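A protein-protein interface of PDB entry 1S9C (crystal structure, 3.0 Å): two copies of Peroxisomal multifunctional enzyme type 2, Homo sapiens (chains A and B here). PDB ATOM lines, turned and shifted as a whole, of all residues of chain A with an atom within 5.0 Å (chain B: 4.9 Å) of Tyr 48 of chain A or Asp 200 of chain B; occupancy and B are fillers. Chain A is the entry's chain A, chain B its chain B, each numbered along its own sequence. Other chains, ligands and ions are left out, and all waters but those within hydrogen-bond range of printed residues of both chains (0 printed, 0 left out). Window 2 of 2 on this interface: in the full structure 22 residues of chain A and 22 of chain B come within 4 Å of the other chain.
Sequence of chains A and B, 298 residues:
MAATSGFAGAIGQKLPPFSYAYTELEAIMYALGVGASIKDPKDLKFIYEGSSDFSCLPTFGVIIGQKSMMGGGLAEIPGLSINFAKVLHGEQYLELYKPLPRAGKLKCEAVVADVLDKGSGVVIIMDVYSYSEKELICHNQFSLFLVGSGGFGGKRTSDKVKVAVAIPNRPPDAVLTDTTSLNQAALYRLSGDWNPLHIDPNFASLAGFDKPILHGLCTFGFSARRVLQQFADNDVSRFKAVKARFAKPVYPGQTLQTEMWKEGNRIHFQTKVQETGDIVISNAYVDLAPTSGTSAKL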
ATOM      1  N   ILE A  28      33.879  -6.219 -35.810  1.00  0.00           N
ATOM      2  CA  ILE A  28      34.086  -6.053 -34.376  1.00  0.00           C
ATOM      3  C   ILE A  28      35.523  -6.389 -34.011  1.00  0.00           C
ATOM      4  O   ILE A  28      36.152  -5.705 -33.197  1.00  0.00           O
ATOM      5  CB  ILE A  28      33.137  -6.947 -33.578  1.00  0.00           C
ATOM      6  CG1 ILE A  28      31.695  -6.538 -33.883  1.00  0.00           C
ATOM      7  CG2 ILE A  28      33.445  -6.853 -32.098  1.00  0.00           C
ATOM      8  CD1 ILE A  28      30.676  -7.456 -33.307  1.00  0.00           C
ATOM      9  N   LEU A  44      29.934   0.840 -27.659  1.00  0.00           N
ATOM     10  CA  LEU A  44      29.144  -0.371 -27.798  1.00  0.00           C
ATOM     11  C   LEU A  44      28.674  -0.458 -29.247  1.00  0.00           C
ATOM     12  O   LEU A  44      28.428  -1.540 -29.782  1.00  0.00           O
ATOM     13  CB  LEU A  44      27.956  -0.296 -26.859  1.00  0.00           C
ATOM     14  CG  LEU A  44      27.260  -1.614 -26.573  1.00  0.00           C
ATOM     15  CD1 LEU A  44      28.216  -2.567 -25.910  1.00  0.00           C
ATOM     16  CD2 LEU A  44      26.063  -1.355 -25.669  1.00  0.00           C
ATOM     17  N   LYS A  45      28.572   0.714 -29.868  1.00  0.00           N
ATOM     18  CA  LYS A  45      28.146   0.884 -31.251  1.00  0.00           C
ATOM     19  C   LYS A  45      29.031   0.141 -32.262  1.00  0.00           C
ATOM     20  O   LYS A  45      28.557  -0.248 -33.330  1.00  0.00           O
ATOM     21  CB  LYS A  45      28.129   2.385 -31.557  1.00  0.00           C
ATOM     22  CG  LYS A  45      27.872   2.750 -32.996  1.00  0.00           C
ATOM     23  CD  LYS A  45      27.798   4.262 -33.188  1.00  0.00           C
ATOM     24  CE  LYS A  45      27.462   4.572 -34.637  1.00  0.00           C
ATOM     25  NZ  LYS A  45      27.196   6.004 -34.871  1.00  0.00           N
ATOM     26  N   PHE A  46      30.310  -0.047 -31.916  1.00  0.00           N
ATOM     27  CA  PHE A  46      31.287  -0.725 -32.780  1.00  0.00           C
ATOM     28  C   PHE A  46      31.685  -2.120 -32.302  1.00  0.00           C
ATOM     29  O   PHE A  46      32.354  -2.854 -33.020  1.00  0.00           O
ATOM     30  CB  PHE A  46      32.562   0.115 -32.884  1.00  0.00           C
ATOM     31  CG  PHE A  46      32.316   1.553 -33.222  1.00  0.00           C
ATOM     32  CD1 PHE A  46      31.790   1.922 -34.457  1.00  0.00           C
ATOM     33  CD2 PHE A  46      32.612   2.548 -32.305  1.00  0.00           C
ATOM     34  CE1 PHE A  46      31.567   3.271 -34.764  1.00  0.00           C
ATOM     35  CE2 PHE A  46      32.392   3.896 -32.602  1.00  0.00           C
ATOM     36  CZ  PHE A  46      31.871   4.255 -33.831  1.00  0.00           C
ATOM     37  N   ILE A  47      31.266  -2.483 -31.100  1.00  0.00           N
ATOM     38  CA  ILE A  47      31.630  -3.768 -30.521  1.00  0.00           C
ATOM     39  C   ILE A  47      30.490  -4.778 -30.438  1.00  0.00           C
ATOM     40  O   ILE A  47      30.723  -5.989 -30.460  1.00  0.00           O
ATOM     41  CB  ILE A  47      32.158  -3.570 -29.099  1.00  0.00           C
ATOM     42  CG1 ILE A  47      33.250  -2.516 -29.091  1.00  0.00           C
ATOM     43  CG2 ILE A  47      32.746  -4.844 -28.573  1.00  0.00           C
ATOM     44  CD1 ILE A  47      33.750  -2.261 -27.699  1.00  0.00           C
ATOM     45  N   TYR A  48      29.261  -4.288 -30.332  1.00  0.00           N
ATOM     46  CA  TYR A  48      28.097  -5.160 -30.221  1.00  0.00           C
ATOM     47  C   TYR A  48      27.199  -5.143 -31.469  1.00  0.00           C
ATOM     48  O   TYR A  48      26.590  -4.126 -31.793  1.00  0.00           O
ATOM     49  CB  TYR A  48      27.317  -4.723 -28.970  1.00  0.00           C
ATOM     50  CG  TYR A  48      26.089  -5.555 -28.680  1.00  0.00           C
ATOM     51  CD1 TYR A  48      26.112  -6.935 -28.832  1.00  0.00           C
ATOM     52  CD2 TYR A  48      24.908  -4.967 -28.255  1.00  0.00           C
ATOM     53  CE1 TYR A  48      24.995  -7.704 -28.569  1.00  0.00           C
ATOM     54  CE2 TYR A  48      23.785  -5.726 -27.988  1.00  0.00           C
ATOM     55  CZ  TYR A  48      23.834  -7.094 -28.146  1.00  0.00           C
ATOM     56  OH  TYR A  48      22.717  -7.854 -27.882  1.00  0.00           O
ATOM     57  N   GLU A  49      27.124  -6.275 -32.165  1.00  0.00           N
ATOM     58  CA  GLU A  49      26.301  -6.383 -33.368  1.00  0.00           C
ATOM     59  C   GLU A  49      24.836  -6.186 -33.031  1.00  0.00           C
ATOM     60  O   GLU A  49      24.053  -5.772 -33.877  1.00  0.00           O
ATOM     61  CB  GLU A  49      26.482  -7.746 -34.034  1.00  0.00           C
ATOM     62  CG  GLU A  49      25.891  -8.934 -33.285  1.00  0.00           C
ATOM     63  CD  GLU A  49      26.627  -9.284 -32.006  1.00  0.00           C
ATOM     64  OE1 GLU A  49      27.803  -8.898 -31.839  1.00  0.00           O
ATOM     65  OE2 GLU A  49      26.024  -9.973 -31.162  1.00  0.00           O
ATOM     66  N   GLY A  50      24.474  -6.485 -31.787  1.00  0.00           N
ATOM     67  CA  GLY A  50      23.099  -6.317 -31.354  1.00  0.00           C
ATOM     68  C   GLY A  50      22.678  -4.866 -31.192  1.00  0.00           C
ATOM     69  O   GLY A  50      21.492  -4.549 -31.173  1.00  0.00           O
ATOM     70  N   SER A  51      23.648  -3.975 -31.061  1.00  0.00           N
ATOM     71  CA  SER A  51      23.332  -2.567 -30.913  1.00  0.00           C
ATOM     72  C   SER A  51      22.522  -2.120 -32.120  1.00  0.00           C
ATOM     73  O   SER A  51      22.846  -2.455 -33.252  1.00  0.00           O
ATOM     74  CB  SER A  51      24.613  -1.747 -30.815  1.00  0.00           C
ATOM     75  OG  SER A  51      24.325  -0.390 -30.526  1.00  0.00           O
ATOM     76  N   PHE A  54      24.716  -0.253 -34.255  1.00  0.00           N
ATOM     77  CA  PHE A  54      25.866  -0.947 -34.814  1.00  0.00           C
ATOM     78  C   PHE A  54      26.342  -0.453 -36.152  1.00  0.00           C
ATOM     79  O   PHE A  54      25.603  -0.430 -37.134  1.00  0.00           O
ATOM     80  CB  PHE A  54      25.626  -2.447 -34.938  1.00  0.00           C
ATOM     81  CG  PHE A  54      26.852  -3.209 -35.359  1.00  0.00           C
ATOM     82  CD1 PHE A  54      27.829  -3.547 -34.428  1.00  0.00           C
ATOM     83  CD2 PHE A  54      27.066  -3.532 -36.694  1.00  0.00           C
ATOM     84  CE1 PHE A  54      29.010  -4.192 -34.814  1.00  0.00           C
ATOM     85  CE2 PHE A  54      28.242  -4.177 -37.096  1.00  0.00           C
ATOM     86  CZ  PHE A  54      29.217  -4.506 -36.151  1.00  0.00           C
ATOM     87  N   ARG B 189      33.434 -13.468 -26.694  1.00  0.00           N
ATOM     88  CA  ARG B 189      32.227 -13.803 -27.417  1.00  0.00           C
ATOM     89  C   ARG B 189      32.505 -14.043 -28.893  1.00  0.00           C
ATOM     90  O   ARG B 189      31.795 -14.823 -29.536  1.00  0.00           O
ATOM     91  CB  ARG B 189      31.155 -12.721 -27.223  1.00  0.00           C
ATOM     92  CG  ARG B 189      31.499 -11.335 -27.724  1.00  0.00           C
ATOM     93  CD  ARG B 189      30.479 -10.322 -27.183  1.00  0.00           C
ATOM     94  NE  ARG B 189      29.113 -10.674 -27.569  1.00  0.00           N
ATOM     95  CZ  ARG B 189      28.501 -10.243 -28.674  1.00  0.00           C
ATOM     96  NH1 ARG B 189      29.114  -9.425 -29.514  1.00  0.00           N
ATOM     97  NH2 ARG B 189      27.278 -10.658 -28.963  1.00  0.00           N
ATOM     98  N   PRO B 196      23.618 -12.078 -25.478  1.00  0.00           N
ATOM     99  CA  PRO B 196      23.613 -10.661 -25.084  1.00  0.00           C
ATOM    100  C   PRO B 196      23.864 -10.470 -23.612  1.00  0.00           C
ATOM    101  O   PRO B 196      24.222  -9.382 -23.177  1.00  0.00           O
ATOM    102  CB  PRO B 196      22.217 -10.188 -25.477  1.00  0.00           C
ATOM    103  CG  PRO B 196      21.835 -11.117 -26.588  1.00  0.00           C
ATOM    104  CD  PRO B 196      22.319 -12.448 -26.062  1.00  0.00           C
ATOM    105  N   LEU B 197      23.661 -11.538 -22.851  1.00  0.00           N
ATOM    106  CA  LEU B 197      23.855 -11.512 -21.409  1.00  0.00           C
ATOM    107  C   LEU B 197      25.262 -11.055 -21.037  1.00  0.00           C
ATOM    108  O   LEU B 197      25.480 -10.512 -19.950  1.00  0.00           O
ATOM    109  CB  LEU B 197      23.612 -12.903 -20.825  1.00  0.00           C
ATOM    110  CG  LEU B 197      23.933 -13.053 -19.340  1.00  0.00           C
ATOM    111  CD1 LEU B 197      23.014 -12.162 -18.517  1.00  0.00           C
ATOM    112  CD2 LEU B 197      23.777 -14.497 -18.939  1.00  0.00           C
ATOM    113  N   HIS B 198      26.210 -11.262 -21.944  1.00  0.00           N
ATOM    114  CA  HIS B 198      27.591 -10.906 -21.682  1.00  0.00           C
ATOM    115  C   HIS B 198      28.032  -9.567 -22.238  1.00  0.00           C
ATOM    116  O   HIS B 198      29.203  -9.220 -22.138  1.00  0.00           O
ATOM    117  CB  HIS B 198      28.501 -12.002 -22.228  1.00  0.00           C
ATOM    118  CG  HIS B 198      28.112 -13.372 -21.786  1.00  0.00           C
ATOM    119  ND1 HIS B 198      28.128 -13.756 -20.463  1.00  0.00           N
ATOM    120  CD2 HIS B 198      27.657 -14.439 -22.483  1.00  0.00           C
ATOM    121  CE1 HIS B 198      27.699 -15.001 -20.364  1.00  0.00           C
ATOM    122  NE2 HIS B 198      27.407 -15.440 -21.577  1.00  0.00           N
ATOM    123  N   ILE B 199      27.122  -8.800 -22.817  1.00  0.00           N
ATOM    124  CA  ILE B 199      27.545  -7.526 -23.367  1.00  0.00           C
ATOM    125  C   ILE B 199      26.476  -6.459 -23.382  1.00  0.00           C
ATOM    126  O   ILE B 199      26.779  -5.263 -23.312  1.00  0.00           O
ATOM    127  CB  ILE B 199      28.104  -7.716 -24.789  1.00  0.00           C
ATOM    128  CG1 ILE B 199      28.712  -6.405 -25.284  1.00  0.00           C
ATOM    129  CG2 ILE B 199      27.014  -8.220 -25.717  1.00  0.00           C
ATOM    130  CD1 ILE B 199      29.468  -6.556 -26.573  1.00  0.00           C
ATOM    131  N   ASP B 200      25.224  -6.886 -23.450  1.00  0.00           N
ATOM    132  CA  ASP B 200      24.110  -5.948 -23.473  1.00  0.00           C
ATOM    133  C   ASP B 200      23.706  -5.554 -22.042  1.00  0.00           C
ATOM    134  O   ASP B 200      23.265  -6.394 -21.261  1.00  0.00           O
ATOM    135  CB  ASP B 200      22.917  -6.585 -24.205  1.00  0.00           C
ATOM    136  CG  ASP B 200      21.836  -5.568 -24.568  1.00  0.00           C
ATOM    137  OD1 ASP B 200      21.717  -4.534 -23.860  1.00  0.00           O
ATOM    138  OD2 ASP B 200      21.099  -5.812 -25.554  1.00  0.00           O
ATOM    139  N   PRO B 201      23.857  -4.267 -21.689  1.00  0.00           N
ATOM    140  CA  PRO B 201      23.517  -3.736 -20.366  1.00  0.00           C
ATOM    141  C   PRO B 201      22.044  -3.935 -20.003  1.00  0.00           C
ATOM    142  O   PRO B 201      21.714  -4.549 -18.982  1.00  0.00           O
ATOM    143  CB  PRO B 201      23.858  -2.261 -20.490  1.00  0.00           C
ATOM    144  CG  PRO B 201      24.952  -2.260 -21.486  1.00  0.00           C
ATOM    145  CD  PRO B 201      24.474  -3.222 -22.518  1.00  0.00           C
ATOM    146  N   ASN B 202      21.155  -3.404 -20.836  1.00  0.00           N
ATOM    147  CA  ASN B 202      19.741  -3.533 -20.563  1.00  0.00           C
ATOM    148  C   ASN B 202      19.419  -5.010 -20.534  1.00  0.00           C
ATOM    149  O   ASN B 202      18.731  -5.485 -19.629  1.00  0.00           O
ATOM    150  CB  ASN B 202      18.910  -2.826 -21.631  1.00  0.00           C
ATOM    151  CG  ASN B 202      17.479  -2.553 -21.178  1.00  0.00           C
ATOM    152  OD1 ASN B 202      17.145  -2.692 -19.999  1.00  0.00           O
ATOM    153  ND2 ASN B 202      16.631  -2.143 -22.110  1.00  0.00           N
ATOM    154  N   PHE B 203      19.934  -5.757 -21.501  1.00  0.00           N
ATOM    155  CA  PHE B 203      19.643  -7.183 -21.519  1.00  0.00           C
ATOM    156  C   PHE B 203      20.085  -7.870 -20.229  1.00  0.00           C
ATOM    157  O   PHE B 203      19.423  -8.792 -19.737  1.00  0.00           O
ATOM    158  CB  PHE B 203      20.304  -7.863 -22.718  1.00  0.00           C
ATOM    159  CG  PHE B 203      19.988  -9.327 -22.822  1.00  0.00           C
ATOM    160  CD1 PHE B 203      20.630 -10.255 -22.004  1.00  0.00           C
ATOM    161  CD2 PHE B 203      19.007  -9.774 -23.697  1.00  0.00           C
ATOM    162  CE1 PHE B 203      20.296 -11.595 -22.056  1.00  0.00           C
ATOM    163  CE2 PHE B 203      18.668 -11.121 -23.752  1.00  0.00           C
ATOM    164  CZ  PHE B 203      19.313 -12.030 -22.930  1.00  0.00           C
ATOM    165  N   ALA B 204      21.203  -7.417 -19.678  1.00  0.00           N
ATOM    166  CA  ALA B 204      21.723  -8.006 -18.454  1.00  0.00           C
ATOM    167  C   ALA B 204      20.871  -7.628 -17.244  1.00  0.00           C
ATOM    168  O   ALA B 204      20.635  -8.460 -16.358  1.00  0.00           O
ATOM    169  CB  ALA B 204      23.155  -7.570 -18.248  1.00  0.00           C
ATOM    170  N   PRO B 212      26.583  -6.618 -17.429  1.00  0.00           N
ATOM    171  CA  PRO B 212      26.858  -7.870 -18.138  1.00  0.00           C
ATOM    172  C   PRO B 212      27.912  -8.704 -17.434  1.00  0.00           C
ATOM    173  O   PRO B 212      28.822  -8.159 -16.808  1.00  0.00           O
ATOM    174  CB  PRO B 212      27.322  -7.395 -19.509  1.00  0.00           C
ATOM    175  CG  PRO B 212      26.541  -6.154 -19.698  1.00  0.00           C
ATOM    176  CD  PRO B 212      26.682  -5.479 -18.354  1.00  0.00           C
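The side-chain carboxylate (OD1) of Asp 200 of chain B sits at hydrogen-bond distance from the backbone NH (N) of Phe 203 of chain B, at 3.2 Å. The side-chain carboxylate (OD1) of Asp 200 of chain B is in hydrogen-bond range of the backbone NH (N) of Asn 202 of chain B (3.3 Å).
Among the printed residues, merely in contact across the chains: Leu 44 of chain A with Ile 199 of chain B, Leu 44 of chain A with Pro 201 of chain B, Ile 47 of chain A with Arg 189 of chain B, Tyr 48 of chain A with Arg 189 of chain B, Tyr 48 of chain A with Pro 196 of chain B and Tyr 48 of chain A with Ile 199 of chain B.
No position is printed for both chains. Of the 8 pairs that touch across the chains among the printed residues, none has its exchanged pair printed and touching as well.
Printed residues of chain A that touch a printed residue of chain B: Leu 44, Ile 47, Tyr 48 and Glu 49. Hydrophobic or aromatic side chains of chain A that line the printed part of chain B: Leu 44 and Tyr 48. Of the 11 printed residues of chain B, 5 touch a printed residue of chain A. Printed residues of chain B that touch a printed residue of chain A: Arg 189, Pro 196, Ile 199, Asp 200 and Pro 201.
The side-chain carboxylate (OE2) of Glu 49 of chain A is in salt-bridge range of the guanidinium group (NH2) of Arg 189 of chain B (2.6 Å). The side-chain hydroxyl (OH) of Tyr 48 of chain A sits at hydrogen-bond distance from the side-chain carboxylate (OD2) of Asp 200 of chain B, 3.5 Å away.
Of chain B, only Arg 189, Pro 196, Ile 199 and Asp 200 come within 4 Å of Tyr 48 of chain A. Of the printed residues of chain A, Arg 189 of chain B touches Ile 47 (3.9 Å), Tyr 48 (3.8 Å) and Glu 49 (2.6 Å). Of the printed residues of chain B, Ile 47 of chain A touches Arg 189. Printed residues of chain B within 4 Å of Glu 49 of chain A: Arg 189. Of the printed residues of chain B, Leu 44 of chain A touches Ile 199 and Pro 201. Of the printed residues of chain A, Pro 196 of chain B touches Tyr 48. Phe 46 of chain A touches none of the printed residues of chain B. The nearest printed residue of chain A that does not touch Asp 200 of chain B is Leu 44 of chain A (5.5 Å). The nearest printed residue of chain B that does not touch Ile 47 of chain A is Ile 199 of chain B (4.1 Å).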
